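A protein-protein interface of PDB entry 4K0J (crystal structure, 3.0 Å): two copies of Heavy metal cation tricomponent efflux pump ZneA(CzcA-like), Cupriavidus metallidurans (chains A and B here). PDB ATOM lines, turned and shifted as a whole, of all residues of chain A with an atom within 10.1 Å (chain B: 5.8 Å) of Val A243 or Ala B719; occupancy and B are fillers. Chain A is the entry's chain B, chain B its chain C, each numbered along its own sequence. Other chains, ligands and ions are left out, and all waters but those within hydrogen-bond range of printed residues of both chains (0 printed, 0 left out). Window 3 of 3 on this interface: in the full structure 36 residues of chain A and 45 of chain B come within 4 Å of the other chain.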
ATOM      1  N   ILE A 197      10.936  22.606 -27.867  1.00  0.00           N
ATOM      2  CA  ILE A 197      10.780  22.047 -26.534  1.00  0.00           C
ATOM      3  C   ILE A 197      10.386  20.588 -26.721  1.00  0.00           C
ATOM      4  O   ILE A 197       9.242  20.277 -27.063  1.00  0.00           O
ATOM      5  CB  ILE A 197       9.731  22.806 -25.694  1.00  0.00           C
ATOM      6  CG1 ILE A 197      10.188  24.239 -25.429  1.00  0.00           C
ATOM      7  CG2 ILE A 197       9.528  22.120 -24.364  1.00  0.00           C
ATOM      8  CD1 ILE A 197      11.264  24.350 -24.361  1.00  0.00           C
ATOM      9  N   GLN A 201      12.337  16.763 -23.314  1.00  0.00           N
ATOM     10  CA  GLN A 201      12.813  17.929 -22.576  1.00  0.00           C
ATOM     11  C   GLN A 201      11.883  18.256 -21.413  1.00  0.00           C
ATOM     12  O   GLN A 201      12.337  18.479 -20.294  1.00  0.00           O
ATOM     13  CB  GLN A 201      12.968  19.143 -23.495  1.00  0.00           C
ATOM     14  CG  GLN A 201      14.326  19.225 -24.169  1.00  0.00           C
ATOM     15  CD  GLN A 201      14.491  20.474 -25.019  1.00  0.00           C
ATOM     16  OE1 GLN A 201      15.468  20.610 -25.761  1.00  0.00           O
ATOM     17  NE2 GLN A 201      13.539  21.395 -24.913  1.00  0.00           N
ATOM     18  N   ILE A 202      10.581  18.273 -21.681  1.00  0.00           N
ATOM     19  CA  ILE A 202       9.593  18.571 -20.652  1.00  0.00           C
ATOM     20  C   ILE A 202       9.622  17.554 -19.512  1.00  0.00           C
ATOM     21  O   ILE A 202       9.637  17.927 -18.338  1.00  0.00           O
ATOM     22  CB  ILE A 202       8.181  18.622 -21.242  1.00  0.00           C
ATOM     23  CG1 ILE A 202       8.134  19.624 -22.389  1.00  0.00           C
ATOM     24  CG2 ILE A 202       7.174  18.995 -20.172  1.00  0.00           C
ATOM     25  CD1 ILE A 202       6.783  19.759 -23.033  1.00  0.00           C
ATOM     26  N   THR A 203       9.633  16.271 -19.865  1.00  0.00           N
ATOM     27  CA  THR A 203       9.633  15.198 -18.872  1.00  0.00           C
ATOM     28  C   THR A 203      10.950  15.125 -18.094  1.00  0.00           C
ATOM     29  O   THR A 203      10.996  14.594 -16.984  1.00  0.00           O
ATOM     30  CB  THR A 203       9.354  13.827 -19.515  1.00  0.00           C
ATOM     31  OG1 THR A 203      10.510  13.388 -20.235  1.00  0.00           O
ATOM     32  CG2 THR A 203       8.169  13.914 -20.462  1.00  0.00           C
ATOM     33  N   GLN A 204      12.019  15.655 -18.682  1.00  0.00           N
ATOM     34  CA  GLN A 204      13.306  15.719 -17.999  1.00  0.00           C
ATOM     35  C   GLN A 204      13.376  16.994 -17.162  1.00  0.00           C
ATOM     36  O   GLN A 204      14.203  17.119 -16.258  1.00  0.00           O
ATOM     37  CB  GLN A 204      14.456  15.672 -19.009  1.00  0.00           C
ATOM     38  CG  GLN A 204      15.839  15.509 -18.392  1.00  0.00           C
ATOM     39  CD  GLN A 204      16.939  15.512 -19.435  1.00  0.00           C
ATOM     40  OE1 GLN A 204      16.680  15.346 -20.628  1.00  0.00           O
ATOM     41  NE2 GLN A 204      18.178  15.704 -18.991  1.00  0.00           N
ATOM     42  N   ALA A 205      12.492  17.937 -17.466  1.00  0.00           N
ATOM     43  CA  ALA A 205      12.450  19.202 -16.748  1.00  0.00           C
ATOM     44  C   ALA A 205      11.755  19.042 -15.407  1.00  0.00           C
ATOM     45  O   ALA A 205      12.332  19.326 -14.361  1.00  0.00           O
ATOM     46  CB  ALA A 205      11.750  20.262 -17.579  1.00  0.00           C
ATOM     47  N   ILE A 206      10.514  18.571 -15.435  1.00  0.00           N
ATOM     48  CA  ILE A 206       9.703  18.552 -14.227  1.00  0.00           C
ATOM     49  C   ILE A 206       9.985  17.338 -13.349  1.00  0.00           C
ATOM     50  O   ILE A 206       9.417  17.195 -12.270  1.00  0.00           O
ATOM     51  CB  ILE A 206       8.203  18.677 -14.544  1.00  0.00           C
ATOM     52  CG1 ILE A 206       7.552  17.309 -14.703  1.00  0.00           C
ATOM     53  CG2 ILE A 206       7.996  19.512 -15.802  1.00  0.00           C
ATOM     54  CD1 ILE A 206       6.040  17.379 -14.737  1.00  0.00           C
ATOM     55  N   SER A 207      10.884  16.477 -13.805  1.00  0.00           N
ATOM     56  CA  SER A 207      11.356  15.367 -12.990  1.00  0.00           C
ATOM     57  C   SER A 207      12.502  15.830 -12.097  1.00  0.00           C
ATOM     58  O   SER A 207      12.973  15.086 -11.237  1.00  0.00           O
ATOM     59  CB  SER A 207      11.814  14.209 -13.882  1.00  0.00           C
ATOM     60  OG  SER A 207      12.570  13.248 -13.159  1.00  0.00           O
ATOM     61  N   GLU A 208      12.940  17.067 -12.295  1.00  0.00           N
ATOM     62  CA  GLU A 208      14.132  17.565 -11.616  1.00  0.00           C
ATOM     63  C   GLU A 208      13.876  18.677 -10.591  1.00  0.00           C
ATOM     64  O   GLU A 208      14.717  18.928  -9.727  1.00  0.00           O
ATOM     65  CB  GLU A 208      15.183  18.007 -12.642  1.00  0.00           C
ATOM     66  CG  GLU A 208      15.745  16.860 -13.470  1.00  0.00           C
ATOM     67  CD  GLU A 208      16.670  17.327 -14.582  1.00  0.00           C
ATOM     68  OE1 GLU A 208      16.796  18.553 -14.785  1.00  0.00           O
ATOM     69  OE2 GLU A 208      17.267  16.463 -15.260  1.00  0.00           O
ATOM     70  N   ASN A 209      12.730  19.346 -10.688  1.00  0.00           N
ATOM     71  CA  ASN A 209      12.366  20.347  -9.683  1.00  0.00           C
ATOM     72  C   ASN A 209      11.312  19.835  -8.696  1.00  0.00           C
ATOM     73  O   ASN A 209      10.300  20.489  -8.426  1.00  0.00           O
ATOM     74  CB  ASN A 209      11.970  21.697 -10.312  1.00  0.00           C
ATOM     75  CG  ASN A 209      10.823  21.580 -11.299  1.00  0.00           C
ATOM     76  OD1 ASN A 209       9.653  21.693 -10.929  1.00  0.00           O
ATOM     77  ND2 ASN A 209      11.156  21.374 -12.569  1.00  0.00           N
ATOM     78  N   ASP A 237      -1.233  23.151  -8.670  1.00  0.00           N
ATOM     79  CA  ASP A 237      -0.762  24.526  -8.723  1.00  0.00           C
ATOM     80  C   ASP A 237       0.740  24.573  -8.934  1.00  0.00           C
ATOM     81  O   ASP A 237       1.220  25.257  -9.837  1.00  0.00           O
ATOM     82  CB  ASP A 237      -1.147  25.266  -7.447  1.00  0.00           C
ATOM     83  CG  ASP A 237      -2.631  25.182  -7.158  1.00  0.00           C
ATOM     84  OD1 ASP A 237      -3.357  26.147  -7.485  1.00  0.00           O
ATOM     85  OD2 ASP A 237      -3.071  24.143  -6.617  1.00  0.00           O
ATOM     86  N   ASP A 238       1.483  23.834  -8.114  1.00  0.00           N
ATOM     87  CA  ASP A 238       2.934  23.784  -8.257  1.00  0.00           C
ATOM     88  C   ASP A 238       3.292  23.065  -9.549  1.00  0.00           C
ATOM     89  O   ASP A 238       4.405  23.186 -10.053  1.00  0.00           O
ATOM     90  CB  ASP A 238       3.586  23.063  -7.077  1.00  0.00           C
ATOM     91  CG  ASP A 238       3.222  23.672  -5.747  1.00  0.00           C
ATOM     92  OD1 ASP A 238       2.179  24.351  -5.669  1.00  0.00           O
ATOM     93  OD2 ASP A 238       3.974  23.459  -4.774  1.00  0.00           O
ATOM     94  N   LEU A 239       2.333  22.310 -10.072  1.00  0.00           N
ATOM     95  CA  LEU A 239       2.502  21.605 -11.333  1.00  0.00           C
ATOM     96  C   LEU A 239       2.310  22.560 -12.502  1.00  0.00           C
ATOM     97  O   LEU A 239       3.215  22.753 -13.315  1.00  0.00           O
ATOM     98  CB  LEU A 239       1.493  20.460 -11.431  1.00  0.00           C
ATOM     99  CG  LEU A 239       1.774  19.363 -12.455  1.00  0.00           C
ATOM    100  CD1 LEU A 239       3.256  19.043 -12.508  1.00  0.00           C
ATOM    101  CD2 LEU A 239       0.986  18.122 -12.095  1.00  0.00           C
ATOM    102  N   GLY A 240       1.131  23.174 -12.570  1.00  0.00           N
ATOM    103  CA  GLY A 240       0.781  24.050 -13.675  1.00  0.00           C
ATOM    104  C   GLY A 240       1.573  25.346 -13.776  1.00  0.00           C
ATOM    105  O   GLY A 240       1.144  26.281 -14.457  1.00  0.00           O
ATOM    106  N   ASN A 241       2.721  25.405 -13.103  1.00  0.00           N
ATOM    107  CA  ASN A 241       3.582  26.586 -13.132  1.00  0.00           C
ATOM    108  C   ASN A 241       5.063  26.233 -13.035  1.00  0.00           C
ATOM    109  O   ASN A 241       5.785  26.785 -12.204  1.00  0.00           O
ATOM    110  CB  ASN A 241       3.205  27.555 -12.007  1.00  0.00           C
ATOM    111  CG  ASN A 241       1.770  28.056 -12.119  1.00  0.00           C
ATOM    112  OD1 ASN A 241       0.833  27.404 -11.654  1.00  0.00           O
ATOM    113  ND2 ASN A 241       1.595  29.217 -12.745  1.00  0.00           N
ATOM    114  N   ILE A 242       5.513  25.316 -13.888  1.00  0.00           N
ATOM    115  CA  ILE A 242       6.911  24.875 -13.890  1.00  0.00           C
ATOM    116  C   ILE A 242       7.670  25.381 -15.119  1.00  0.00           C
ATOM    117  O   ILE A 242       7.153  25.356 -16.239  1.00  0.00           O
ATOM    118  CB  ILE A 242       7.024  23.332 -13.799  1.00  0.00           C
ATOM    119  CG1 ILE A 242       6.358  22.826 -12.517  1.00  0.00           C
ATOM    120  CG2 ILE A 242       8.479  22.883 -13.845  1.00  0.00           C
ATOM    121  CD1 ILE A 242       6.405  21.327 -12.348  1.00  0.00           C
ATOM    122  N   VAL A 243       8.901  25.839 -14.898  1.00  0.00           N
ATOM    123  CA  VAL A 243       9.722  26.425 -15.952  1.00  0.00           C
ATOM    124  C   VAL A 243      10.227  25.393 -16.956  1.00  0.00           C
ATOM    125  O   VAL A 243      10.964  24.481 -16.594  1.00  0.00           O
ATOM    126  CB  VAL A 243      10.926  27.167 -15.355  1.00  0.00           C
ATOM    127  CG1 VAL A 243      11.870  27.625 -16.457  1.00  0.00           C
ATOM    128  CG2 VAL A 243      10.456  28.343 -14.508  1.00  0.00           C
ATOM    129  N   VAL A 244       9.828  25.558 -18.216  1.00  0.00           N
ATOM    130  CA  VAL A 244      10.230  24.669 -19.307  1.00  0.00           C
ATOM    131  C   VAL A 244      11.748  24.537 -19.425  1.00  0.00           C
ATOM    132  O   VAL A 244      12.258  23.859 -20.320  1.00  0.00           O
ATOM    133  CB  VAL A 244       9.671  25.166 -20.652  1.00  0.00           C
ATOM    134  CG1 VAL A 244       8.154  25.136 -20.634  1.00  0.00           C
ATOM    135  CG2 VAL A 244      10.175  26.574 -20.948  1.00  0.00           C
ATOM    136  N   ASP A 256       0.838  27.764 -18.613  1.00  0.00           N
ATOM    137  CA  ASP A 256      -0.473  27.739 -19.252  1.00  0.00           C
ATOM    138  C   ASP A 256      -0.661  26.445 -20.035  1.00  0.00           C
ATOM    139  O   ASP A 256      -0.987  25.405 -19.459  1.00  0.00           O
ATOM    140  CB  ASP A 256      -0.644  28.949 -20.178  1.00  0.00           C
ATOM    141  CG  ASP A 256      -0.436  30.269 -19.460  1.00  0.00           C
ATOM    142  OD1 ASP A 256      -1.410  30.801 -18.889  1.00  0.00           O
ATOM    143  OD2 ASP A 256       0.704  30.776 -19.467  1.00  0.00           O
ATOM    144  N   ASP B 715       8.809  30.335  -3.985  1.00  0.00           N
ATOM    145  CA  ASP B 715       7.641  30.999  -4.549  1.00  0.00           C
ATOM    146  C   ASP B 715       7.491  30.558  -5.997  1.00  0.00           C
ATOM    147  O   ASP B 715       8.331  30.865  -6.846  1.00  0.00           O
ATOM    148  CB  ASP B 715       7.796  32.523  -4.448  1.00  0.00           C
ATOM    149  CG  ASP B 715       6.524  33.282  -4.811  1.00  0.00           C
ATOM    150  OD1 ASP B 715       5.868  32.927  -5.819  1.00  0.00           O
ATOM    151  OD2 ASP B 715       6.195  34.260  -4.093  1.00  0.00           O
ATOM    152  N   ARG B 716       6.416  29.824  -6.266  1.00  0.00           N
ATOM    153  CA  ARG B 716       6.171  29.279  -7.593  1.00  0.00           C
ATOM    154  C   ARG B 716       5.967  30.378  -8.630  1.00  0.00           C
ATOM    155  O   ARG B 716       6.757  30.506  -9.563  1.00  0.00           O
ATOM    156  CB  ARG B 716       4.968  28.334  -7.570  1.00  0.00           C
ATOM    157  CG  ARG B 716       5.216  27.028  -6.822  1.00  0.00           C
ATOM    158  CD  ARG B 716       6.146  26.099  -7.596  1.00  0.00           C
ATOM    159  NE  ARG B 716       6.591  24.970  -6.782  1.00  0.00           N
ATOM    160  CZ  ARG B 716       7.216  23.899  -7.261  1.00  0.00           C
ATOM    161  NH1 ARG B 716       7.585  22.923  -6.441  1.00  0.00           N
ATOM    162  NH2 ARG B 716       7.467  23.797  -8.559  1.00  0.00           N
ATOM    163  N   ALA B 717       4.915  31.173  -8.455  1.00  0.00           N
ATOM    164  CA  ALA B 717       4.599  32.254  -9.386  1.00  0.00           C
ATOM    165  C   ALA B 717       5.727  33.282  -9.557  1.00  0.00           C
ATOM    166  O   ALA B 717       5.875  33.876 -10.630  1.00  0.00           O
ATOM    167  CB  ALA B 717       3.305  32.946  -8.975  1.00  0.00           C
ATOM    168  N   ALA B 718       6.518  33.497  -8.509  1.00  0.00           N
ATOM    169  CA  ALA B 718       7.639  34.426  -8.612  1.00  0.00           C
ATOM    170  C   ALA B 718       8.681  33.917  -9.594  1.00  0.00           C
ATOM    171  O   ALA B 718       9.141  34.660 -10.455  1.00  0.00           O
ATOM    172  CB  ALA B 718       8.268  34.669  -7.260  1.00  0.00           C
ATOM    173  N   ALA B 719       9.046  32.644  -9.459  1.00  0.00           N
ATOM    174  CA  ALA B 719      10.024  32.020 -10.344  1.00  0.00           C
ATOM    175  C   ALA B 719       9.371  31.645 -11.668  1.00  0.00           C
ATOM    176  O   ALA B 719      10.035  31.183 -12.597  1.00  0.00           O
ATOM    177  CB  ALA B 719      10.642  30.799  -9.681  1.00  0.00           C
ATOM    178  N   ALA B 720       8.061  31.837 -11.739  1.00  0.00           N
ATOM    179  CA  ALA B 720       7.323  31.637 -12.969  1.00  0.00           C
ATOM    180  C   ALA B 720       7.313  32.945 -13.743  1.00  0.00           C
ATOM    181  O   ALA B 720       7.043  32.972 -14.943  1.00  0.00           O
ATOM    182  CB  ALA B 720       5.906  31.187 -12.666  1.00  0.00           C
ATOM    183  N   ARG B 721       7.612  34.034 -13.043  1.00  0.00           N
ATOM    184  CA  ARG B 721       7.686  35.347 -13.667  1.00  0.00           C
ATOM    185  C   ARG B 721       9.129  35.810 -13.806  1.00  0.00           C
ATOM    186  O   ARG B 721       9.388  36.909 -14.295  1.00  0.00           O
ATOM    187  CB  ARG B 721       6.877  36.372 -12.870  1.00  0.00           C
ATOM    188  CG  ARG B 721       5.381  36.139 -12.927  1.00  0.00           C
ATOM    189  CD  ARG B 721       4.624  37.156 -12.101  1.00  0.00           C
ATOM    190  NE  ARG B 721       4.370  36.705 -10.735  1.00  0.00           N
ATOM    191  CZ  ARG B 721       5.113  37.033  -9.682  1.00  0.00           C
ATOM    192  NH1 ARG B 721       4.796  36.575  -8.478  1.00  0.00           N
ATOM    193  NH2 ARG B 721       6.169  37.820  -9.830  1.00  0.00           N
ATOM    194  N   LEU B 722      10.066  34.967 -13.374  1.00  0.00           N
ATOM    195  CA  LEU B 722      11.485  35.290 -13.476  1.00  0.00           C
ATOM    196  C   LEU B 722      12.252  34.196 -14.202  1.00  0.00           C
ATOM    197  O   LEU B 722      13.465  34.303 -14.391  1.00  0.00           O
ATOM    198  CB  LEU B 722      12.103  35.518 -12.093  1.00  0.00           C
ATOM    199  CG  LEU B 722      11.605  36.706 -11.266  1.00  0.00           C
ATOM    200  CD1 LEU B 722      12.503  36.941 -10.063  1.00  0.00           C
ATOM    201  CD2 LEU B 722      11.512  37.962 -12.118  1.00  0.00           C
ATOM    202  N   GLY B 723      11.544  33.146 -14.604  1.00  0.00           N
ATOM    203  CA  GLY B 723      12.166  32.027 -15.288  1.00  0.00           C
ATOM    204  C   GLY B 723      13.269  31.388 -14.463  1.00  0.00           C
ATOM    205  O   GLY B 723      14.453  31.543 -14.771  1.00  0.00           O
ATOM    206  N   ILE B 724      12.875  30.684 -13.403  1.00  0.00           N
ATOM    207  CA  ILE B 724      13.816  29.994 -12.522  1.00  0.00           C
ATOM    208  C   ILE B 724      13.214  28.679 -12.035  1.00  0.00           C
ATOM    209  O   ILE B 724      12.019  28.612 -11.734  1.00  0.00           O
ATOM    210  CB  ILE B 724      14.221  30.876 -11.309  1.00  0.00           C
ATOM    211  CG1 ILE B 724      15.311  31.869 -11.715  1.00  0.00           C
ATOM    212  CG2 ILE B 724      14.689  30.019 -10.127  1.00  0.00           C
ATOM    213  CD1 ILE B 724      16.218  32.294 -10.580  1.00  0.00           C
ATOM    214  N   ASN B 725      14.037  27.634 -11.985  1.00  0.00           N
ATOM    215  CA  ASN B 725      13.614  26.338 -11.469  1.00  0.00           C
ATOM    216  C   ASN B 725      13.822  26.237  -9.969  1.00  0.00           C
ATOM    217  O   ASN B 725      14.787  26.776  -9.429  1.00  0.00           O
ATOM    218  CB  ASN B 725      14.399  25.213 -12.137  1.00  0.00           C
ATOM    219  CG  ASN B 725      14.209  25.178 -13.632  1.00  0.00           C
ATOM    220  OD1 ASN B 725      13.091  25.285 -14.130  1.00  0.00           O
ATOM    221  ND2 ASN B 725      15.307  25.025 -14.362  1.00  0.00           N
ATOM    222  N   VAL B 726      12.930  25.525  -9.296  1.00  0.00           N
ATOM    223  CA  VAL B 726      13.113  25.282  -7.878  1.00  0.00           C
ATOM    224  C   VAL B 726      14.370  24.442  -7.677  1.00  0.00           C
ATOM    225  O   VAL B 726      15.013  24.511  -6.634  1.00  0.00           O
ATOM    226  CB  VAL B 726      11.878  24.597  -7.249  1.00  0.00           C
ATOM    227  CG1 VAL B 726      10.676  24.746  -8.167  1.00  0.00           C
ATOM    228  CG2 VAL B 726      12.154  23.126  -6.958  1.00  0.00           C
ATOM    229  N   VAL B 787      12.356  35.218  -4.929  1.00  0.00           N
ATOM    230  CA  VAL B 787      11.517  34.106  -5.368  1.00  0.00           C
ATOM    231  C   VAL B 787      11.351  33.022  -4.306  1.00  0.00           C
ATOM    232  O   VAL B 787      10.823  31.946  -4.589  1.00  0.00           O
ATOM    233  CB  VAL B 787      12.091  33.431  -6.639  1.00  0.00           C
ATOM    234  CG1 VAL B 787      11.798  34.260  -7.883  1.00  0.00           C
ATOM    235  CG2 VAL B 787      13.585  33.171  -6.482  1.00  0.00           C
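The backbone carbonyl oxygen (O) of Val A243 lies close to the side-chain amide oxygen (OD1) of Asn B725.
The side-chain carboxylate (OD2) of Asp A238 lies within salt-bridge range of the guanidinium group (NE) of Arg B716 (3.6 Å).
No position is printed for both chains.
Of the 6 pairs that touch across the chains among the printed residues, none has its exchanged pair printed and touching as well.
Of the 19 printed residues of chain A, 3 touch a printed residue of chain B.
Hydrophobic or aromatic side chains of chain A that line the printed part of chain B: Val A243.
Of the 13 printed residues of chain B, 5 touch a printed residue of chain A.
The backbone carbonyl oxygen (O) of Ala A205 sits at hydrogen-bond distance from the side-chain amide nitrogen (ND2) of Asn A209, at 3.0 Å.
N of Ile B724 is in hydrogen-bond range of O of Ala B719, at 3.0 Å.
Among the printed residues, pairs that only touch across the chains: Asn A209 with Arg B716, Asn A209 with Val B726, Val A243 with Ala B719 and Val A243 with Ile B724.
Of chain B, only Ala B719 (3.4 Å), Ile B724 (3.2 Å) and Asn B725 (3.1 Å) come within 4 Å of Val A243.
Ala B719 touches one residue of chain A.
No residue of chain A comes within 4 Å of Ala B717.
No residue of chain A comes within 4 Å of Ala B720.
Gly B723 touches none of the printed residues of chain A.
Ile B724 touches just one residue of chain A: Val A243.
Asn B725 touches one residue of chain A.
Of the printed residues of chain B, Asn A209 touches Arg B716 and Val B726.
Printed residues of chain A within 4 Å of Val B726: Asn A209 (3.5 Å).
The nearest residue of chain A that does not touch Ala B719 is Asn A241 (6.1 Å).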
